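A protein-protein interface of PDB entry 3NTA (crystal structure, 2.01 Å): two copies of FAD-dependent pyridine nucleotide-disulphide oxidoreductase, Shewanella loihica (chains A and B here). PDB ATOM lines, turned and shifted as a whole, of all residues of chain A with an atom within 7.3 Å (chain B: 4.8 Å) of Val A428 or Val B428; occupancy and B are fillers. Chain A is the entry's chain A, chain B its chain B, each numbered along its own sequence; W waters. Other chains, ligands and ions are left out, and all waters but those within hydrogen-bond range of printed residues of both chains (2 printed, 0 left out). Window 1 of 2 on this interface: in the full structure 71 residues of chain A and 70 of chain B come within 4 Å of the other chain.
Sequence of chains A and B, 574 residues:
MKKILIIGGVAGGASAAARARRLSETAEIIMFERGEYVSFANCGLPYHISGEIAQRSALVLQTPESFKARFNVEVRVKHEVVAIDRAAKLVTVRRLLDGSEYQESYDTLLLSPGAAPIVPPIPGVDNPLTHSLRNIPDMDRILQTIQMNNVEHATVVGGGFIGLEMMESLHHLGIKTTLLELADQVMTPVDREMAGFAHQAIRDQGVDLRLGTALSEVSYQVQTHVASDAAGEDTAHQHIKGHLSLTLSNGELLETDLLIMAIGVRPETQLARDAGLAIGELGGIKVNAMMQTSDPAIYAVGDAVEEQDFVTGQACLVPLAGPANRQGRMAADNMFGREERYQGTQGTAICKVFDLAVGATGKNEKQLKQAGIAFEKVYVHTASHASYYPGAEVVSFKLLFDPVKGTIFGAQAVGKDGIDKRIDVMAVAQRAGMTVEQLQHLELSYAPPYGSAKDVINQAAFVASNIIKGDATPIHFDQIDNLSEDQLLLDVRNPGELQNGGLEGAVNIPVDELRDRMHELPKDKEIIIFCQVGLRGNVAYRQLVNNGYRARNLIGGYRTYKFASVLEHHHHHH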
ATOM      1  N   GLN A 346     -36.428   0.278 -11.934  1.00  0.00           N
ATOM      2  CA  GLN A 346     -35.934   0.160 -13.314  1.00  0.00           C
ATOM      3  C   GLN A 346     -35.631  -1.300 -13.681  1.00  0.00           C
ATOM      4  O   GLN A 346     -35.582  -1.673 -14.871  1.00  0.00           O
ATOM      5  CB  GLN A 346     -34.681   1.015 -13.513  1.00  0.00           C
ATOM      6  CG  GLN A 346     -34.933   2.506 -13.634  1.00  0.00           C
ATOM      7  CD  GLN A 346     -33.605   3.314 -13.470  1.00  0.00           C
ATOM      8  OE1 GLN A 346     -33.073   3.485 -12.304  1.00  0.00           O
ATOM      9  NE2 GLN A 346     -33.023   3.734 -14.582  1.00  0.00           N
ATOM     10  N   THR A 348     -32.770  -2.675 -12.624  1.00  0.00           N
ATOM     11  CA  THR A 348     -31.381  -2.747 -13.012  1.00  0.00           C
ATOM     12  C   THR A 348     -30.853  -4.089 -12.489  1.00  0.00           C
ATOM     13  O   THR A 348     -31.072  -4.361 -11.294  1.00  0.00           O
ATOM     14  CB  THR A 348     -30.566  -1.520 -12.424  1.00  0.00           C
ATOM     15  OG1 THR A 348     -31.209  -0.269 -12.759  1.00  0.00           O
ATOM     16  CG2 THR A 348     -29.149  -1.568 -12.988  1.00  0.00           C
ATOM     17  N   THR A 361     -30.952  -2.703 -17.849  1.00  0.00           N
ATOM     18  CA  THR A 361     -31.819  -1.876 -17.040  1.00  0.00           C
ATOM     19  C   THR A 361     -33.033  -1.374 -17.830  1.00  0.00           C
ATOM     20  O   THR A 361     -32.881  -1.213 -18.935  1.00  0.00           O
ATOM     21  CB  THR A 361     -30.979  -0.627 -16.624  1.00  0.00           C
ATOM     22  OG1 THR A 361     -31.727   0.150 -15.702  1.00  0.00           O
ATOM     23  CG2 THR A 361     -30.592   0.288 -17.874  1.00  0.00           C
ATOM     24  N   ILE A 408     -35.415   7.317 -23.332  1.00  0.00           N
ATOM     25  CA  ILE A 408     -34.662   6.097 -23.083  1.00  0.00           C
ATOM     26  C   ILE A 408     -35.517   5.055 -22.469  1.00  0.00           C
ATOM     27  O   ILE A 408     -35.936   5.219 -21.329  1.00  0.00           O
ATOM     28  CB  ILE A 408     -33.389   6.337 -22.156  1.00  0.00           C
ATOM     29  CG1 ILE A 408     -32.468   7.354 -22.881  1.00  0.00           C
ATOM     30  CG2 ILE A 408     -32.682   4.971 -21.782  1.00  0.00           C
ATOM     31  CD1 ILE A 408     -31.322   8.007 -21.885  1.00  0.00           C
ATOM     32  N   ARG A 422     -21.109   0.333 -17.877  1.00  0.00           N
ATOM     33  CA  ARG A 422     -22.138   0.747 -18.917  1.00  0.00           C
ATOM     34  C   ARG A 422     -23.564   0.693 -18.486  1.00  0.00           C
ATOM     35  O   ARG A 422     -24.296   1.620 -18.713  1.00  0.00           O
ATOM     36  CB  ARG A 422     -21.883  -0.112 -20.265  1.00  0.00           C
ATOM     37  CG  ARG A 422     -20.714   0.449 -21.178  1.00  0.00           C
ATOM     38  CD  ARG A 422     -19.599   1.078 -20.390  1.00  0.00           C
ATOM     39  NE  ARG A 422     -18.421   1.491 -21.113  1.00  0.00           N
ATOM     40  CZ  ARG A 422     -17.277   0.845 -21.065  1.00  0.00           C
ATOM     41  NH1 ARG A 422     -17.161  -0.249 -20.374  1.00  0.00           N
ATOM     42  NH2 ARG A 422     -16.238   1.305 -21.713  1.00  0.00           N
ATOM     43  N   ILE A 423     -23.978  -0.270 -17.706  1.00  0.00           N
ATOM     44  CA  ILE A 423     -25.335  -0.404 -17.245  1.00  0.00           C
ATOM     45  C   ILE A 423     -25.527   0.636 -16.145  1.00  0.00           C
ATOM     46  O   ILE A 423     -26.573   1.319 -16.143  1.00  0.00           O
ATOM     47  CB  ILE A 423     -25.578  -1.850 -16.702  1.00  0.00           C
ATOM     48  CG1 ILE A 423     -25.517  -2.882 -17.902  1.00  0.00           C
ATOM     49  CG2 ILE A 423     -27.031  -1.934 -16.018  1.00  0.00           C
ATOM     50  CD1 ILE A 423     -26.522  -2.429 -18.930  1.00  0.00           C
ATOM     51  N   ASP A 424     -24.512   0.889 -15.284  1.00  0.00           N
ATOM     52  CA  ASP A 424     -24.689   1.992 -14.262  1.00  0.00           C
ATOM     53  C   ASP A 424     -24.895   3.359 -14.851  1.00  0.00           C
ATOM     54  O   ASP A 424     -25.820   4.057 -14.516  1.00  0.00           O
ATOM     55  CB  ASP A 424     -23.524   2.061 -13.174  1.00  0.00           C
ATOM     56  CG  ASP A 424     -23.532   0.854 -12.231  1.00  0.00           C
ATOM     57  OD1 ASP A 424     -24.552   0.149 -12.355  1.00  0.00           O
ATOM     58  OD2 ASP A 424     -22.630   0.636 -11.408  1.00  0.00           O
ATOM     59  N   VAL A 425     -24.030   3.733 -15.793  1.00  0.00           N
ATOM     60  CA  VAL A 425     -24.239   4.964 -16.578  1.00  0.00           C
ATOM     61  C   VAL A 425     -25.632   5.114 -17.206  1.00  0.00           C
ATOM     62  O   VAL A 425     -26.296   6.204 -17.166  1.00  0.00           O
ATOM     63  CB  VAL A 425     -23.107   5.078 -17.576  1.00  0.00           C
ATOM     64  CG1 VAL A 425     -23.340   6.287 -18.588  1.00  0.00           C
ATOM     65  CG2 VAL A 425     -21.797   5.380 -16.805  1.00  0.00           C
ATOM     66  N   MET A 426     -26.084   4.050 -17.879  1.00  0.00           N
ATOM     67  CA  MET A 426     -27.458   4.082 -18.518  1.00  0.00           C
ATOM     68  C   MET A 426     -28.477   4.097 -17.388  1.00  0.00           C
ATOM     69  O   MET A 426     -29.498   4.753 -17.451  1.00  0.00           O
ATOM     70  CB  MET A 426     -27.664   2.768 -19.344  1.00  0.00           C
ATOM     71  CG  MET A 426     -27.006   2.744 -20.694  1.00  0.00           C
ATOM     72  SD  MET A 426     -26.976   4.411 -21.652  1.00  0.00           S
ATOM     73  CE  MET A 426     -28.869   4.624 -21.889  1.00  0.00           C
ATOM     74  N   ALA A 427     -28.272   3.333 -16.322  1.00  0.00           N
ATOM     75  CA  ALA A 427     -29.297   3.521 -15.259  1.00  0.00           C
ATOM     76  C   ALA A 427     -29.430   4.954 -14.715  1.00  0.00           C
ATOM     77  O   ALA A 427     -30.584   5.429 -14.405  1.00  0.00           O
ATOM     78  CB  ALA A 427     -29.138   2.482 -14.109  1.00  0.00           C
ATOM     79  N   VAL A 428     -28.295   5.628 -14.555  1.00  0.00           N
ATOM     80  CA  VAL A 428     -28.279   6.994 -14.051  1.00  0.00           C
ATOM     81  C   VAL A 428     -28.930   7.906 -15.075  1.00  0.00           C
ATOM     82  O   VAL A 428     -29.903   8.599 -14.779  1.00  0.00           O
ATOM     83  CB  VAL A 428     -26.845   7.479 -13.776  1.00  0.00           C
ATOM     84  CG1 VAL A 428     -26.852   8.941 -13.354  1.00  0.00           C
ATOM     85  CG2 VAL A 428     -26.186   6.613 -12.713  1.00  0.00           C
ATOM     86  N   ALA A 429     -28.389   7.893 -16.288  1.00  0.00           N
ATOM     87  CA  ALA A 429     -29.007   8.669 -17.440  1.00  0.00           C
ATOM     88  C   ALA A 429     -30.509   8.489 -17.600  1.00  0.00           C
ATOM     89  O   ALA A 429     -31.220   9.452 -17.817  1.00  0.00           O
ATOM     90  CB  ALA A 429     -28.330   8.284 -18.772  1.00  0.00           C
ATOM     91  N   GLN A 430     -31.019   7.262 -17.466  1.00  0.00           N
ATOM     92  CA  GLN A 430     -32.487   7.129 -17.667  1.00  0.00           C
ATOM     93  C   GLN A 430     -33.229   7.722 -16.484  1.00  0.00           C
ATOM     94  O   GLN A 430     -34.155   8.545 -16.634  1.00  0.00           O
ATOM     95  CB  GLN A 430     -32.921   5.649 -17.911  1.00  0.00           C
ATOM     96  CG  GLN A 430     -34.509   5.395 -17.864  1.00  0.00           C
ATOM     97  CD  GLN A 430     -34.741   3.813 -17.916  1.00  0.00           C
ATOM     98  OE1 GLN A 430     -34.335   3.037 -16.989  1.00  0.00           O
ATOM     99  NE2 GLN A 430     -35.218   3.336 -19.062  1.00  0.00           N
ATOM    100  N   ARG A 431     -32.773   7.385 -15.289  1.00  0.00           N
ATOM    101  CA  ARG A 431     -33.444   7.879 -14.038  1.00  0.00           C
ATOM    102  C   ARG A 431     -33.435   9.367 -14.009  1.00  0.00           C
ATOM    103  O   ARG A 431     -34.378  10.019 -13.583  1.00  0.00           O
ATOM    104  CB  ARG A 431     -32.827   7.358 -12.715  1.00  0.00           C
ATOM    105  CG  ARG A 431     -33.595   7.881 -11.433  1.00  0.00           C
ATOM    106  CD  ARG A 431     -33.314   6.920 -10.257  1.00  0.00           C
ATOM    107  NE  ARG A 431     -33.906   5.607 -10.321  1.00  0.00           N
ATOM    108  CZ  ARG A 431     -35.079   5.206  -9.826  1.00  0.00           C
ATOM    109  NH1 ARG A 431     -35.940   5.993  -9.209  1.00  0.00           N
ATOM    110  NH2 ARG A 431     -35.398   3.910  -9.978  1.00  0.00           N
ATOM    111  N   ALA A 432     -32.407   9.952 -14.515  1.00  0.00           N
ATOM    112  CA  ALA A 432     -32.406  11.457 -14.482  1.00  0.00           C
ATOM    113  C   ALA A 432     -33.157  12.057 -15.630  1.00  0.00           C
ATOM    114  O   ALA A 432     -33.142  13.297 -15.765  1.00  0.00           O
ATOM    115  CB  ALA A 432     -30.897  12.022 -14.488  1.00  0.00           C
ATOM    116  N   GLY A 433     -33.774  11.216 -16.522  1.00  0.00           N
ATOM    117  CA  GLY A 433     -34.571  11.760 -17.631  1.00  0.00           C
ATOM    118  C   GLY A 433     -33.830  12.261 -18.862  1.00  0.00           C
ATOM    119  O   GLY A 433     -34.368  13.096 -19.598  1.00  0.00           O
ATOM    120  N   MET A 434     -32.603  11.823 -19.137  1.00  0.00           N
ATOM    121  CA  MET A 434     -31.813  12.260 -20.359  1.00  0.00           C
ATOM    122  C   MET A 434     -32.363  11.567 -21.633  1.00  0.00           C
ATOM    123  O   MET A 434     -32.832  10.461 -21.581  1.00  0.00           O
ATOM    124  CB  MET A 434     -30.392  11.815 -20.215  1.00  0.00           C
ATOM    125  CG  MET A 434     -29.721  12.592 -19.130  1.00  0.00           C
ATOM    126  SD  MET A 434     -27.780  12.059 -19.078  1.00  0.00           S
ATOM    127  CE  MET A 434     -27.270  12.345 -20.571  1.00  0.00           C
ATOM    128  N   LEU A 439     -27.259  11.972 -24.815  1.00  0.00           N
ATOM    129  CA  LEU A 439     -26.322  10.989 -24.453  1.00  0.00           C
ATOM    130  C   LEU A 439     -25.073  11.176 -25.205  1.00  0.00           C
ATOM    131  O   LEU A 439     -24.008  10.715 -24.684  1.00  0.00           O
ATOM    132  CB  LEU A 439     -26.769   9.467 -24.493  1.00  0.00           C
ATOM    133  CG  LEU A 439     -27.814   8.757 -23.666  1.00  0.00           C
ATOM    134  CD1 LEU A 439     -28.110   7.449 -24.286  1.00  0.00           C
ATOM    135  CD2 LEU A 439     -27.176   8.493 -22.259  1.00  0.00           C
ATOM    136  N   LEU A 442     -22.140  13.123 -23.178  1.00  0.00           N
ATOM    137  CA  LEU A 442     -21.434  12.548 -22.002  1.00  0.00           C
ATOM    138  C   LEU A 442     -19.876  12.618 -22.046  1.00  0.00           C
ATOM    139  O   LEU A 442     -19.266  12.315 -23.073  1.00  0.00           O
ATOM    140  CB  LEU A 442     -21.965  11.143 -21.692  1.00  0.00           C
ATOM    141  CG  LEU A 442     -23.366  11.013 -21.134  1.00  0.00           C
ATOM    142  CD1 LEU A 442     -23.606   9.516 -20.836  1.00  0.00           C
ATOM    143  CD2 LEU A 442     -23.759  11.750 -19.819  1.00  0.00           C
ATOM    144  N   GLU A 443     -19.256  13.200 -20.966  1.00  0.00           N
ATOM    145  CA  GLU A 443     -17.760  13.402 -20.780  1.00  0.00           C
ATOM    146  C   GLU A 443     -17.330  12.356 -19.728  1.00  0.00           C
ATOM    147  O   GLU A 443     -17.471  12.591 -18.500  1.00  0.00           O
ATOM    148  CB  GLU A 443     -17.407  14.858 -20.232  1.00  0.00           C
ATOM    149  CG  GLU A 443     -15.909  15.279 -20.274  1.00  0.00           C
ATOM    150  CD  GLU A 443     -15.596  16.576 -19.566  1.00  0.00           C
ATOM    151  OE1 GLU A 443     -16.663  17.316 -19.641  1.00  0.00           O
ATOM    152  OE2 GLU A 443     -14.513  16.858 -19.011  1.00  0.00           O
ATOM    153  N   LEU A 444     -16.826  11.204 -20.173  1.00  0.00           N
ATOM    154  CA  LEU A 444     -16.582  10.084 -19.234  1.00  0.00           C
ATOM    155  C   LEU A 444     -15.078  10.006 -18.960  1.00  0.00           C
ATOM    156  O   LEU A 444     -14.310  10.735 -19.559  1.00  0.00           O
ATOM    157  CB  LEU A 444     -17.262   8.760 -19.729  1.00  0.00           C
ATOM    158  CG  LEU A 444     -18.865   8.813 -19.919  1.00  0.00           C
ATOM    159  CD1 LEU A 444     -19.419   7.427 -20.318  1.00  0.00           C
ATOM    160  CD2 LEU A 444     -19.674   9.351 -18.729  1.00  0.00           C
ATOM    161  N   ILE A 457     -20.947   4.069 -24.773  1.00  0.00           N
ATOM    162  CA  ILE A 457     -22.193   4.886 -24.664  1.00  0.00           C
ATOM    163  C   ILE A 457     -22.197   6.069 -25.652  1.00  0.00           C
ATOM    164  O   ILE A 457     -23.282   6.413 -26.175  1.00  0.00           O
ATOM    165  CB  ILE A 457     -22.425   5.438 -23.136  1.00  0.00           C
ATOM    166  CG1 ILE A 457     -22.366   4.325 -22.024  1.00  0.00           C
ATOM    167  CG2 ILE A 457     -23.754   6.184 -22.967  1.00  0.00           C
ATOM    168  CD1 ILE A 457     -23.135   3.127 -22.372  1.00  0.00           C
ATOM    169  N   ASP B 424     -17.593   7.927 -13.571  1.00  0.00           N
ATOM    170  CA  ASP B 424     -18.568   8.021 -14.764  1.00  0.00           C
ATOM    171  C   ASP B 424     -19.978   8.264 -14.238  1.00  0.00           C
ATOM    172  O   ASP B 424     -20.656   9.112 -14.721  1.00  0.00           O
ATOM    173  CB  ASP B 424     -18.541   6.711 -15.645  1.00  0.00           C
ATOM    174  CG  ASP B 424     -17.133   6.456 -16.366  1.00  0.00           C
ATOM    175  OD1 ASP B 424     -16.382   7.474 -16.593  1.00  0.00           O
ATOM    176  OD2 ASP B 424     -16.868   5.262 -16.612  1.00  0.00           O
ATOM    177  N   VAL B 425     -20.427   7.535 -13.213  1.00  0.00           N
ATOM    178  CA  VAL B 425     -21.749   7.809 -12.624  1.00  0.00           C
ATOM    179  C   VAL B 425     -21.988   9.279 -12.164  1.00  0.00           C
ATOM    180  O   VAL B 425     -23.021   9.918 -12.470  1.00  0.00           O
ATOM    181  CB  VAL B 425     -22.098   6.688 -11.541  1.00  0.00           C
ATOM    182  CG1 VAL B 425     -23.221   7.152 -10.659  1.00  0.00           C
ATOM    183  CG2 VAL B 425     -22.459   5.358 -12.267  1.00  0.00           C
ATOM    184  N   MET B 426     -21.021   9.813 -11.399  1.00  0.00           N
ATOM    185  CA  MET B 426     -21.071  11.239 -10.934  1.00  0.00           C
ATOM    186  C   MET B 426     -20.997  12.175 -12.165  1.00  0.00           C
ATOM    187  O   MET B 426     -21.710  13.176 -12.264  1.00  0.00           O
ATOM    188  CB  MET B 426     -19.913  11.517  -9.887  1.00  0.00           C
ATOM    189  CG  MET B 426     -20.094  10.829  -8.557  1.00  0.00           C
ATOM    190  SD  MET B 426     -21.800  11.119  -7.767  1.00  0.00           S
ATOM    191  CE  MET B 426     -22.026  12.980  -7.985  1.00  0.00           C
ATOM    192  N   ALA B 427     -20.134  11.925 -13.143  1.00  0.00           N
ATOM    193  CA  ALA B 427     -20.142  12.784 -14.336  1.00  0.00           C
ATOM    194  C   ALA B 427     -21.512  12.752 -15.044  1.00  0.00           C
ATOM    195  O   ALA B 427     -21.997  13.828 -15.453  1.00  0.00           O
ATOM    196  CB  ALA B 427     -19.035  12.463 -15.253  1.00  0.00           C
ATOM    197  N   VAL B 428     -22.151  11.590 -15.117  1.00  0.00           N
ATOM    198  CA  VAL B 428     -23.505  11.504 -15.657  1.00  0.00           C
ATOM    199  C   VAL B 428     -24.508  12.274 -14.791  1.00  0.00           C
ATOM    200  O   VAL B 428     -25.311  13.056 -15.300  1.00  0.00           O
ATOM    201  CB  VAL B 428     -23.969  10.041 -15.789  1.00  0.00           C
ATOM    202  CG1 VAL B 428     -25.381   9.981 -16.349  1.00  0.00           C
ATOM    203  CG2 VAL B 428     -23.005   9.257 -16.666  1.00  0.00           C
ATOM    204  N   ALA B 429     -24.454  12.043 -13.482  1.00  0.00           N
ATOM    205  CA  ALA B 429     -25.351  12.688 -12.526  1.00  0.00           C
ATOM    206  C   ALA B 429     -25.264  14.222 -12.524  1.00  0.00           C
ATOM    207  O   ALA B 429     -26.302  14.934 -12.513  1.00  0.00           O
ATOM    208  CB  ALA B 429     -25.289  12.066 -11.049  1.00  0.00           C
ATOM    209  N   GLN B 430     -24.053  14.753 -12.644  1.00  0.00           N
ATOM    210  CA  GLN B 430     -23.917  16.183 -12.609  1.00  0.00           C
ATOM    211  C   GLN B 430     -24.338  16.764 -13.935  1.00  0.00           C
ATOM    212  O   GLN B 430     -25.039  17.834 -13.971  1.00  0.00           O
ATOM    213  CB  GLN B 430     -22.436  16.586 -12.238  1.00  0.00           C
ATOM    214  CG  GLN B 430     -22.146  18.039 -12.487  1.00  0.00           C
ATOM    215  CD  GLN B 430     -20.639  18.462 -12.180  1.00  0.00           C
ATOM    216  OE1 GLN B 430     -20.355  19.214 -11.167  1.00  0.00           O
ATOM    217  NE2 GLN B 430     -19.698  18.013 -13.042  1.00  0.00           N
ATOM    218  N   ARG B 431     -23.892  16.135 -15.055  1.00  0.00           N
ATOM    219  CA  ARG B 431     -24.318  16.712 -16.428  1.00  0.00           C
ATOM    220  C   ARG B 431     -25.825  16.685 -16.638  1.00  0.00           C
ATOM    221  O   ARG B 431     -26.456  17.483 -17.337  1.00  0.00           O
ATOM    222  CB  ARG B 431     -23.588  16.051 -17.588  1.00  0.00           C
ATOM    223  CG  ARG B 431     -23.865  16.635 -19.035  1.00  0.00           C
ATOM    224  CD  ARG B 431     -22.912  16.139 -19.998  1.00  0.00           C
ATOM    225  NE  ARG B 431     -21.575  16.636 -19.798  1.00  0.00           N
ATOM    226  CZ  ARG B 431     -21.099  17.767 -20.290  1.00  0.00           C
ATOM    227  NH1 ARG B 431     -21.837  18.565 -21.069  1.00  0.00           N
ATOM    228  NH2 ARG B 431     -19.828  18.115 -20.035  1.00  0.00           N
ATOM    229  N   ALA B 432     -26.472  15.787 -15.988  1.00  0.00           N
ATOM    230  CA  ALA B 432     -27.942  15.706 -16.139  1.00  0.00           C
ATOM    231  C   ALA B 432     -28.637  16.653 -15.138  1.00  0.00           C
ATOM    232  O   ALA B 432     -29.843  16.752 -15.117  1.00  0.00           O
ATOM    233  CB  ALA B 432     -28.359  14.223 -15.887  1.00  0.00           C
ATOM    234  N   MET B 434     -28.818  16.385 -11.681  1.00  0.00           N
ATOM    235  CA  MET B 434     -29.297  15.799 -10.458  1.00  0.00           C
ATOM    236  C   MET B 434     -28.692  16.514  -9.224  1.00  0.00           C
ATOM    237  O   MET B 434     -27.618  17.103  -9.333  1.00  0.00           O
ATOM    238  CB  MET B 434     -28.784  14.350 -10.376  1.00  0.00           C
ATOM    239  CG  MET B 434     -29.493  13.421 -11.382  1.00  0.00           C
ATOM    240  SD  MET B 434     -28.977  11.618 -11.066  1.00  0.00           S
ATOM    241  CE  MET B 434     -29.683  11.228  -9.520  1.00  0.00           C
ATOM    242  N   LEU B 442     -30.610   6.417  -6.744  1.00  0.00           N
ATOM    243  CA  LEU B 442     -29.905   5.655  -7.798  1.00  0.00           C
ATOM    244  C   LEU B 442     -30.006   4.152  -7.599  1.00  0.00           C
ATOM    245  O   LEU B 442     -29.836   3.667  -6.447  1.00  0.00           O
ATOM    246  CB  LEU B 442     -28.446   6.080  -7.941  1.00  0.00           C
ATOM    247  CG  LEU B 442     -28.281   7.388  -8.692  1.00  0.00           C
ATOM    248  CD1 LEU B 442     -26.847   7.417  -9.068  1.00  0.00           C
ATOM    249  CD2 LEU B 442     -29.099   7.558  -9.966  1.00  0.00           C
ATOM    250  N   LEU B 444     -28.513   0.838  -8.897  1.00  0.00           N
ATOM    251  CA  LEU B 444     -27.355   0.467  -9.725  1.00  0.00           C
ATOM    252  C   LEU B 444     -27.263  -1.111  -9.889  1.00  0.00           C
ATOM    253  O   LEU B 444     -28.125  -1.844  -9.386  1.00  0.00           O
ATOM    254  CB  LEU B 444     -26.043   1.127  -9.249  1.00  0.00           C
ATOM    255  CG  LEU B 444     -26.079   2.690  -9.367  1.00  0.00           C
ATOM    256  CD1 LEU B 444     -24.740   3.408  -8.923  1.00  0.00           C
ATOM    257  CD2 LEU B 444     -26.618   3.218 -10.783  1.00  0.00           C
HETATM  258  O   HOH W   1     -20.834  13.839 -18.398  1.00  0.00           O
HETATM  259  O   HOH W   2     -18.054   4.000 -19.370  1.00  0.00           O
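Among the printed residues, merely in contact across the chains: Val A428 with Val B428, Leu A444 with Asp B424, Val A425 with Val B428, Asp A424 with Leu B444, Asp A424 with Val B425, Glu A443 with Ala B427, Ala A432 with Ala B432, Val A428 with Val B425, Thr A348 with Leu B444, Ala A429 with Val B428, Ala A432 with Met B434, Val A425 with Asp B424, Val A428 with Leu B442, Met A434 with Ala B432, Leu A444 with Val B428, Val A428 with Ala B429 and Val A428 with Leu B444.
Gln A346 touches none of the printed residues of chain B. Of the printed residues of chain B, Thr A348 touches Leu B444. Val A428 touches just these residues of chain B: Val B425, Val B428, Ala B429, Leu B442 and Leu B444. Printed residues of chain B within 4 Å of Ala A429: Val B428 (3.7 Å). Printed residues of chain A within 4 Å of Asp B424: Val A425 (3.7 Å) and Leu A444 (3.5 Å). Of the printed residues of chain A, Ala B427 touches Glu A443. Val B428 touches just these residues of chain A: Val A425, Val A428, Ala A429 and Leu A444. Of the printed residues of chain A, Met B434 touches Ala A432. Printed residues of chain A within 4 Å of Leu B444: Thr A348 (3.7 Å), Asp A424 (3.6 Å) and Val A428 (3.9 Å). The nearest residue of chain B that does not touch Val A428 is Met B434 (4.1 Å). The nearest printed residue of chain A that does not touch Met B434 is Val A428 (4.1 Å).
OG1 of Thr A361 is in hydrogen-bond range of OG1 of Thr A348 (3.0 Å). O of Ala A429 lies within hydrogen-bond range of N of Met A434, 3.0 Å away. The backbone carbonyl oxygen of Ala B429 is in hydrogen-bond range of the backbone NH of Met B434, at 3.0 Å.
Asp A424 touches Val B425, and with the chains exchanged Val A425 touches Asp B424. Asp A424 touches Leu B444, and with the chains exchanged Leu A444 touches Asp B424. Val A425 touches Val B428, and with the chains exchanged Val A428 touches Val B425. Val A428 touches Leu B444, and with the chains exchanged Leu A444 touches Val B428. 12 positions are printed for both chains. Of the 18 pairs that touch across the chains among the printed residues, 14 have their exchanged pair printed and touching as well.
OE1 of Glu A443 is in salt-bridge range of NH2 of Arg B431 (3.3 Å).
Printed residues of chain A that touch a printed residue of chain B: Thr A348, Asp A424, Val A425, Val A428, Ala A429, Ala A432, Met A434, Glu A443 and Leu A444. Hydrophobic or aromatic side chains of chain A that line the printed part of chain B: Val A425, Val A428, Ala A432, Met A434 and Leu A444. Of the 12 printed residues of chain B, 10 touch a printed residue of chain A. Hydrophobic or aromatic side chains of chain B that line the printed part of chain A: Val B425, Ala B427, Val B428, Ala B432, Met B434, Leu B442 and Leu B444. Along chain B the printed residues that touch a printed residue of chain A span positions 424 to 444.
Water W2 bridges the guanidinium group of Arg A422 and the side-chain carboxylate of Asp B424. Water W1 lies within hydrogen-bond range of the backbone NH (N) of Glu A443 (3.1 Å), the backbone carbonyl oxygen (O) of Ala B427 (3.2 Å) and the guanidinium group (NE) of Arg B431 (3.2 Å).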
